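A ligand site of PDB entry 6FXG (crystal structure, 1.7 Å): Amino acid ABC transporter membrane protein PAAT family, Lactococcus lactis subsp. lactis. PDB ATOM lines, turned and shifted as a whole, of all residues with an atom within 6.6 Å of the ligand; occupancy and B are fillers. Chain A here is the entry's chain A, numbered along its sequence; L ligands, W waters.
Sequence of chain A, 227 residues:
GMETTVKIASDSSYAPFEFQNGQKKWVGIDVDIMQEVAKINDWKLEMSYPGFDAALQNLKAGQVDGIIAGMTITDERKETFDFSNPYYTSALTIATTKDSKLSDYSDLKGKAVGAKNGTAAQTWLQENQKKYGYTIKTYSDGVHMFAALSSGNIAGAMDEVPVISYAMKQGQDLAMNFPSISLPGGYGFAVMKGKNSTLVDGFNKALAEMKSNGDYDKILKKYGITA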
ATOM      1  N   ASP A  11      36.729  13.633 -22.042  1.00  0.00           N
ATOM      2  CA  ASP A  11      36.605  14.336 -23.303  1.00  0.00           C
ATOM      3  C   ASP A  11      37.970  14.872 -23.718  1.00  0.00           C
ATOM      4  O   ASP A  11      38.909  14.918 -22.942  1.00  0.00           O
ATOM      5  CB  ASP A  11      35.599  15.493 -23.141  1.00  0.00           C
ATOM      6  CG  ASP A  11      34.959  15.964 -24.446  1.00  0.00           C
ATOM      7  OD1 ASP A  11      35.374  15.567 -25.580  1.00  0.00           O
ATOM      8  OD2 ASP A  11      33.984  16.739 -24.303  1.00  0.00           O
ATOM      9  N   SER A  13      38.336  17.990 -25.527  1.00  0.00           N
ATOM     10  CA  SER A  13      38.406  19.463 -25.511  1.00  0.00           C
ATOM     11  C   SER A  13      37.130  19.948 -24.852  1.00  0.00           C
ATOM     12  O   SER A  13      36.073  19.932 -25.481  1.00  0.00           O
ATOM     13  CB  SER A  13      38.572  20.034 -26.904  1.00  0.00           C
ATOM     14  OG  SER A  13      38.588  21.455 -26.853  1.00  0.00           O
ATOM     15  N   TYR A  14      37.210  20.288 -23.559  1.00  0.00           N
ATOM     16  CA  TYR A  14      36.023  20.658 -22.803  1.00  0.00           C
ATOM     17  C   TYR A  14      36.412  21.589 -21.674  1.00  0.00           C
ATOM     18  O   TYR A  14      36.113  21.358 -20.492  1.00  0.00           O
ATOM     19  CB  TYR A  14      35.282  19.425 -22.291  1.00  0.00           C
ATOM     20  CG  TYR A  14      33.789  19.573 -22.188  1.00  0.00           C
ATOM     21  CD1 TYR A  14      33.029  19.961 -23.282  1.00  0.00           C
ATOM     22  CD2 TYR A  14      33.126  19.283 -21.012  1.00  0.00           C
ATOM     23  CE1 TYR A  14      31.654  20.069 -23.184  1.00  0.00           C
ATOM     24  CE2 TYR A  14      31.745  19.379 -20.913  1.00  0.00           C
ATOM     25  CZ  TYR A  14      31.036  19.799 -21.996  1.00  0.00           C
ATOM     26  OH  TYR A  14      29.677  19.874 -21.950  1.00  0.00           O
ATOM     27  N   GLU A  18      38.307  19.737 -18.936  1.00  0.00           N
ATOM     28  CA  GLU A  18      39.530  19.081 -19.416  1.00  0.00           C
ATOM     29  C   GLU A  18      39.927  19.721 -20.734  1.00  0.00           C
ATOM     30  O   GLU A  18      39.077  19.894 -21.610  1.00  0.00           O
ATOM     31  CB  GLU A  18      39.379  17.560 -19.601  1.00  0.00           C
ATOM     32  CG  GLU A  18      38.130  17.160 -20.369  1.00  0.00           C
ATOM     33  CD  GLU A  18      36.926  16.936 -19.489  1.00  0.00           C
ATOM     34  OE1 GLU A  18      37.049  16.920 -18.216  1.00  0.00           O
ATOM     35  OE2 GLU A  18      35.812  16.809 -20.061  1.00  0.00           O
ATOM     36  N   PHE A  52      34.301  12.598 -25.842  1.00  0.00           N
ATOM     37  CA  PHE A  52      33.244  12.127 -24.958  1.00  0.00           C
ATOM     38  C   PHE A  52      32.601  10.827 -25.454  1.00  0.00           C
ATOM     39  O   PHE A  52      32.565   9.824 -24.725  1.00  0.00           O
ATOM     40  CB  PHE A  52      32.180  13.211 -24.757  1.00  0.00           C
ATOM     41  CG  PHE A  52      31.125  12.780 -23.816  1.00  0.00           C
ATOM     42  CD1 PHE A  52      31.436  12.588 -22.464  1.00  0.00           C
ATOM     43  CD2 PHE A  52      29.848  12.516 -24.266  1.00  0.00           C
ATOM     44  CE1 PHE A  52      30.490  12.150 -21.592  1.00  0.00           C
ATOM     45  CE2 PHE A  52      28.875  12.084 -23.382  1.00  0.00           C
ATOM     46  CZ  PHE A  52      29.212  11.902 -22.024  1.00  0.00           C
ATOM     47  N   ALA A  69      34.008  13.719 -17.266  1.00  0.00           N
ATOM     48  CA  ALA A  69      33.983  14.478 -18.527  1.00  0.00           C
ATOM     49  C   ALA A  69      32.838  15.456 -18.570  1.00  0.00           C
ATOM     50  O   ALA A  69      32.082  15.520 -19.542  1.00  0.00           O
ATOM     51  CB  ALA A  69      33.886  13.520 -19.701  1.00  0.00           C
ATOM     52  N   GLY A  70      32.679  16.239 -17.501  1.00  0.00           N
ATOM     53  CA  GLY A  70      31.548  17.138 -17.426  1.00  0.00           C
ATOM     54  C   GLY A  70      30.239  16.427 -17.722  1.00  0.00           C
ATOM     55  O   GLY A  70      29.386  16.977 -18.417  1.00  0.00           O
ATOM     56  N   MET A  71      30.041  15.249 -17.163  1.00  0.00           N
ATOM     57  CA  MET A  71      28.984  14.353 -17.614  1.00  0.00           C
ATOM     58  C   MET A  71      27.762  14.496 -16.739  1.00  0.00           C
ATOM     59  O   MET A  71      27.793  14.160 -15.540  1.00  0.00           O
ATOM     60  CB  MET A  71      29.463  12.900 -17.629  1.00  0.00           C
ATOM     61  CG  MET A  71      28.422  11.933 -18.114  1.00  0.00           C
ATOM     62  SD  MET A  71      29.110  10.298 -18.299  1.00  0.00           S
ATOM     63  CE  MET A  71      27.649   9.414 -18.805  1.00  0.00           C
ATOM     64  N   THR A  72      26.660  14.986 -17.324  1.00  0.00           N
ATOM     65  CA  THR A  72      25.451  15.212 -16.547  1.00  0.00           C
ATOM     66  C   THR A  72      24.810  13.906 -16.094  1.00  0.00           C
ATOM     67  O   THR A  72      24.579  12.980 -16.890  1.00  0.00           O
ATOM     68  CB  THR A  72      24.422  16.009 -17.353  1.00  0.00           C
ATOM     69  OG1 THR A  72      25.035  17.201 -17.858  1.00  0.00           O
ATOM     70  CG2 THR A  72      23.216  16.347 -16.469  1.00  0.00           C
ATOM     71  N   ILE A  73      24.478  13.875 -14.802  1.00  0.00           N
ATOM     72  CA  ILE A  73      23.688  12.792 -14.219  1.00  0.00           C
ATOM     73  C   ILE A  73      22.237  12.975 -14.636  1.00  0.00           C
ATOM     74  O   ILE A  73      21.623  14.032 -14.405  1.00  0.00           O
ATOM     75  CB  ILE A  73      23.809  12.835 -12.689  1.00  0.00           C
ATOM     76  CG1 ILE A  73      25.293  12.723 -12.254  1.00  0.00           C
ATOM     77  CG2 ILE A  73      22.941  11.749 -12.100  1.00  0.00           C
ATOM     78  CD1 ILE A  73      25.497  12.983 -10.751  1.00  0.00           C
ATOM     79  N   ARG A  77      20.275   8.053 -17.952  1.00  0.00           N
ATOM     80  CA  ARG A  77      21.644   7.557 -17.876  1.00  0.00           C
ATOM     81  C   ARG A  77      21.848   6.578 -16.736  1.00  0.00           C
ATOM     82  O   ARG A  77      22.685   5.664 -16.855  1.00  0.00           O
ATOM     83  CB  ARG A  77      22.611   8.707 -17.745  1.00  0.00           C
ATOM     84  CG  ARG A  77      22.950   9.333 -19.079  1.00  0.00           C
ATOM     85  CD  ARG A  77      23.820  10.596 -18.972  1.00  0.00           C
ATOM     86  NE  ARG A  77      24.451  10.895 -20.258  1.00  0.00           N
ATOM     87  CZ  ARG A  77      25.121  12.024 -20.537  1.00  0.00           C
ATOM     88  NH1 ARG A  77      25.250  12.970 -19.640  1.00  0.00           N
ATOM     89  NH2 ARG A  77      25.679  12.204 -21.738  1.00  0.00           N
ATOM     90  N   SER A  90      24.931  21.645 -13.755  1.00  0.00           N
ATOM     91  CA  SER A  90      24.789  21.375 -15.181  1.00  0.00           C
ATOM     92  C   SER A  90      23.696  22.267 -15.759  1.00  0.00           C
ATOM     93  O   SER A  90      22.615  22.363 -15.181  1.00  0.00           O
ATOM     94  CB  SER A  90      24.455  19.905 -15.429  1.00  0.00           C
ATOM     95  OG  SER A  90      24.179  19.636 -16.815  1.00  0.00           O
ATOM     96  N   LEU A  92      22.404  23.739 -19.914  1.00  0.00           N
ATOM     97  CA  LEU A  92      22.616  23.750 -21.351  1.00  0.00           C
ATOM     98  C   LEU A  92      22.097  25.054 -21.933  1.00  0.00           C
ATOM     99  O   LEU A  92      21.119  25.628 -21.449  1.00  0.00           O
ATOM    100  CB  LEU A  92      21.881  22.586 -22.013  1.00  0.00           C
ATOM    101  CG  LEU A  92      22.296  21.157 -21.646  1.00  0.00           C
ATOM    102  CD1 LEU A  92      21.308  20.236 -22.283  1.00  0.00           C
ATOM    103  CD2 LEU A  92      23.691  20.842 -22.136  1.00  0.00           C
ATOM    104  N   LYS A 116      26.952  17.234 -29.544  1.00  0.00           N
ATOM    105  CA  LYS A 116      27.913  16.142 -29.595  1.00  0.00           C
ATOM    106  C   LYS A 116      27.238  14.786 -29.402  1.00  0.00           C
ATOM    107  O   LYS A 116      26.303  14.637 -28.605  1.00  0.00           O
ATOM    108  CB  LYS A 116      28.990  16.370 -28.528  1.00  0.00           C
ATOM    109  CG  LYS A 116      29.893  17.544 -28.876  1.00  0.00           C
ATOM    110  CD  LYS A 116      30.502  18.227 -27.685  1.00  0.00           C
ATOM    111  CE  LYS A 116      31.496  17.327 -26.924  1.00  0.00           C
ATOM    112  NZ  LYS A 116      32.076  18.039 -25.750  1.00  0.00           N
ATOM    113  N   GLY A 118      26.182  11.308 -28.134  1.00  0.00           N
ATOM    114  CA  GLY A 118      26.156  10.708 -26.805  1.00  0.00           C
ATOM    115  C   GLY A 118      25.782  11.617 -25.664  1.00  0.00           C
ATOM    116  O   GLY A 118      25.686  11.119 -24.530  1.00  0.00           O
ATOM    117  N   THR A 119      25.517  12.905 -25.908  1.00  0.00           N
ATOM    118  CA  THR A 119      25.426  13.906 -24.850  1.00  0.00           C
ATOM    119  C   THR A 119      24.005  14.176 -24.403  1.00  0.00           C
ATOM    120  O   THR A 119      23.015  13.832 -25.061  1.00  0.00           O
ATOM    121  CB  THR A 119      26.054  15.250 -25.273  1.00  0.00           C
ATOM    122  OG1 THR A 119      25.362  15.815 -26.400  1.00  0.00           O
ATOM    123  CG2 THR A 119      27.524  15.094 -25.619  1.00  0.00           C
ATOM    124  N   ALA A 120      23.921  14.781 -23.208  1.00  0.00           N
ATOM    125  CA  ALA A 120      22.653  15.287 -22.702  1.00  0.00           C
ATOM    126  C   ALA A 120      22.083  16.343 -23.629  1.00  0.00           C
ATOM    127  O   ALA A 120      20.864  16.431 -23.797  1.00  0.00           O
ATOM    128  CB  ALA A 120      22.838  15.826 -21.273  1.00  0.00           C
ATOM    129  N   ALA A 121      22.955  17.129 -24.264  1.00  0.00           N
ATOM    130  CA  ALA A 121      22.528  18.107 -25.276  1.00  0.00           C
ATOM    131  C   ALA A 121      21.819  17.432 -26.438  1.00  0.00           C
ATOM    132  O   ALA A 121      20.767  17.896 -26.915  1.00  0.00           O
ATOM    133  CB  ALA A 121      23.745  18.895 -25.782  1.00  0.00           C
ATOM    134  N   ASP A 159      25.312  23.097 -25.804  1.00  0.00           N
ATOM    135  CA  ASP A 159      26.369  22.609 -24.922  1.00  0.00           C
ATOM    136  C   ASP A 159      26.219  23.276 -23.569  1.00  0.00           C
ATOM    137  O   ASP A 159      25.306  24.065 -23.343  1.00  0.00           O
ATOM    138  CB  ASP A 159      27.746  22.883 -25.517  1.00  0.00           C
ATOM    139  CG  ASP A 159      28.800  21.887 -25.050  1.00  0.00           C
ATOM    140  OD1 ASP A 159      28.576  21.131 -24.037  1.00  0.00           O
ATOM    141  OD2 ASP A 159      29.861  21.844 -25.721  1.00  0.00           O
ATOM    142  N   GLU A 160      27.115  22.904 -22.637  1.00  0.00           N
ATOM    143  CA  GLU A 160      27.066  23.438 -21.287  1.00  0.00           C
ATOM    144  C   GLU A 160      27.446  24.910 -21.218  1.00  0.00           C
ATOM    145  O   GLU A 160      28.467  25.342 -21.773  1.00  0.00           O
ATOM    146  CB  GLU A 160      28.020  22.655 -20.392  1.00  0.00           C
ATOM    147  CG  GLU A 160      27.460  21.293 -20.028  1.00  0.00           C
ATOM    148  CD  GLU A 160      26.427  21.381 -18.937  1.00  0.00           C
ATOM    149  OE1 GLU A 160      26.621  22.220 -18.028  1.00  0.00           O
ATOM    150  OE2 GLU A 160      25.443  20.610 -18.968  1.00  0.00           O
ATOM    151  N   LEU A 183      19.812  21.285 -15.743  1.00  0.00           N
ATOM    152  CA  LEU A 183      19.729  19.834 -15.574  1.00  0.00           C
ATOM    153  C   LEU A 183      20.073  19.498 -14.117  1.00  0.00           C
ATOM    154  O   LEU A 183      21.254  19.555 -13.734  1.00  0.00           O
ATOM    155  CB  LEU A 183      20.678  19.127 -16.547  1.00  0.00           C
ATOM    156  CG  LEU A 183      20.439  19.374 -18.047  1.00  0.00           C
ATOM    157  CD1 LEU A 183      21.390  18.593 -18.908  1.00  0.00           C
ATOM    158  CD2 LEU A 183      19.008  19.043 -18.439  1.00  0.00           C
ATOM    159  N   TYR A 187      26.998  17.344 -12.626  1.00  0.00           N
ATOM    160  CA  TYR A 187      28.000  16.473 -13.235  1.00  0.00           C
ATOM    161  C   TYR A 187      28.395  15.376 -12.253  1.00  0.00           C
ATOM    162  O   TYR A 187      28.595  15.655 -11.067  1.00  0.00           O
ATOM    163  CB  TYR A 187      29.299  17.198 -13.614  1.00  0.00           C
ATOM    164  CG  TYR A 187      29.212  18.347 -14.620  1.00  0.00           C
ATOM    165  CD1 TYR A 187      28.095  18.587 -15.386  1.00  0.00           C
ATOM    166  CD2 TYR A 187      30.294  19.198 -14.754  1.00  0.00           C
ATOM    167  CE1 TYR A 187      28.060  19.677 -16.286  1.00  0.00           C
ATOM    168  CE2 TYR A 187      30.263  20.265 -15.627  1.00  0.00           C
ATOM    169  CZ  TYR A 187      29.152  20.487 -16.387  1.00  0.00           C
ATOM    170  OH  TYR A 187      29.150  21.572 -17.233  1.00  0.00           O
HETATM  171  N1  LIG L   1      28.282  17.627 -20.887  1.00  0.00           N
HETATM  172  C1  LIG L   1      28.215  16.456 -21.793  1.00  0.00           C
HETATM  173  C2  LIG L   1      27.110  15.497 -21.354  1.00  0.00           C
HETATM  174  O1  LIG L   1      26.719  15.450 -20.154  1.00  0.00           O
HETATM  175  C3  LIG L   1      29.576  15.733 -21.835  1.00  0.00           C
HETATM  176  C4  LIG L   1      30.586  16.428 -22.727  1.00  0.00           C
HETATM  177  O2  LIG L   1      30.239  17.032 -23.787  1.00  0.00           O
HETATM  178  N2  LIG L   1      31.825  16.381 -22.313  1.00  0.00           N
HETATM  179  O   HOH W   1      25.617  18.366 -20.316  1.00  0.00           O
HETATM  180  O   HOH W   2      27.911  18.545 -24.603  1.00  0.00           O
HETATM  181  O   HOH W   3      25.489  17.857 -23.132  1.00  0.00           O
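The backbone carbonyl oxygen of Gly 70 lies within hydrogen-bond range of a nitrogen (N1) of the ligand (2.8 Å). The side-chain hydroxyl (OH) of Tyr 14 lies within hydrogen-bond range of a nitrogen (N1) of the ligand, at 2.9 Å. N of Thr 72 sits at hydrogen-bond distance from O1 of the ligand, 2.9 Å away. O1 of the ligand lies within hydrogen-bond range of OG1 of Thr 72 (3.3 Å). The side-chain amino group of Lys 116 is in hydrogen-bond range of an oxygen (O2) of the ligand, at 2.9 Å. The backbone carbonyl oxygen (O) of Ala 69 sits at hydrogen-bond distance from a nitrogen (N2) of the ligand, 2.9 Å away. O1 of the ligand lies within hydrogen-bond range of NH1 of Arg 77 (2.9 Å). The side-chain carboxylate (OD2) of Asp 11 sits at hydrogen-bond distance from a nitrogen (N2) of the ligand.
OH of Tyr 14 lies within hydrogen-bond range of OD1 of Asp 159 (2.7 Å). NZ of Lys 116 is in salt-bridge range of OD2 of Asp 11 (2.7 Å). O of Lys 116 is in hydrogen-bond range of OG1 of Thr 119. The guanidinium group (NH2) of Arg 77 sits at hydrogen-bond distance from the backbone carbonyl oxygen (O) of Gly 118. OD1 of Asp 11 sits at hydrogen-bond distance from N of Phe 52. OG1 of Thr 119 lies close to N of Ala 121 (3.5 Å). OE1 of Glu 160 is in hydrogen-bond range of OH of Tyr 187, at 2.7 Å. The side-chain hydroxyl (OG) of Ser 90 sits at hydrogen-bond distance from the side-chain carboxylate (OE2) of Glu 160, at 2.7 Å.
Residues that only touch the ligand: Phe 52 (3.7 Å), Met 71 (3.6 Å), Thr 119 (3.8 Å), Ala 120 (3.8 Å) and Glu 160 (3.9 Å). Hydrophobic or aromatic side chains that line the ligand: Tyr 14 and Phe 52. 12 residues have an atom within 4 Å of the ligand: Asp 11, Tyr 14, Phe 52, Ala 69, Gly 70, Met 71, Thr 72, Arg 77, Lys 116, Thr 119, Ala 120 and Glu 160. The nearest printed residue that does not touch the ligand is Asp 159 (4.4 Å).
Water W1 lies within hydrogen-bond range of the side-chain carboxylate of Glu 160 (2.6 Å), the side-chain hydroxyl of Thr 72 (2.8 Å) and a nitrogen (N1) of the ligand (2.8 Å). Water W2 lies within hydrogen-bond range of the side-chain carboxylate (OD1) of Asp 159, an oxygen (O2) of the ligand and the side-chain hydroxyl (OH) of Tyr 14.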
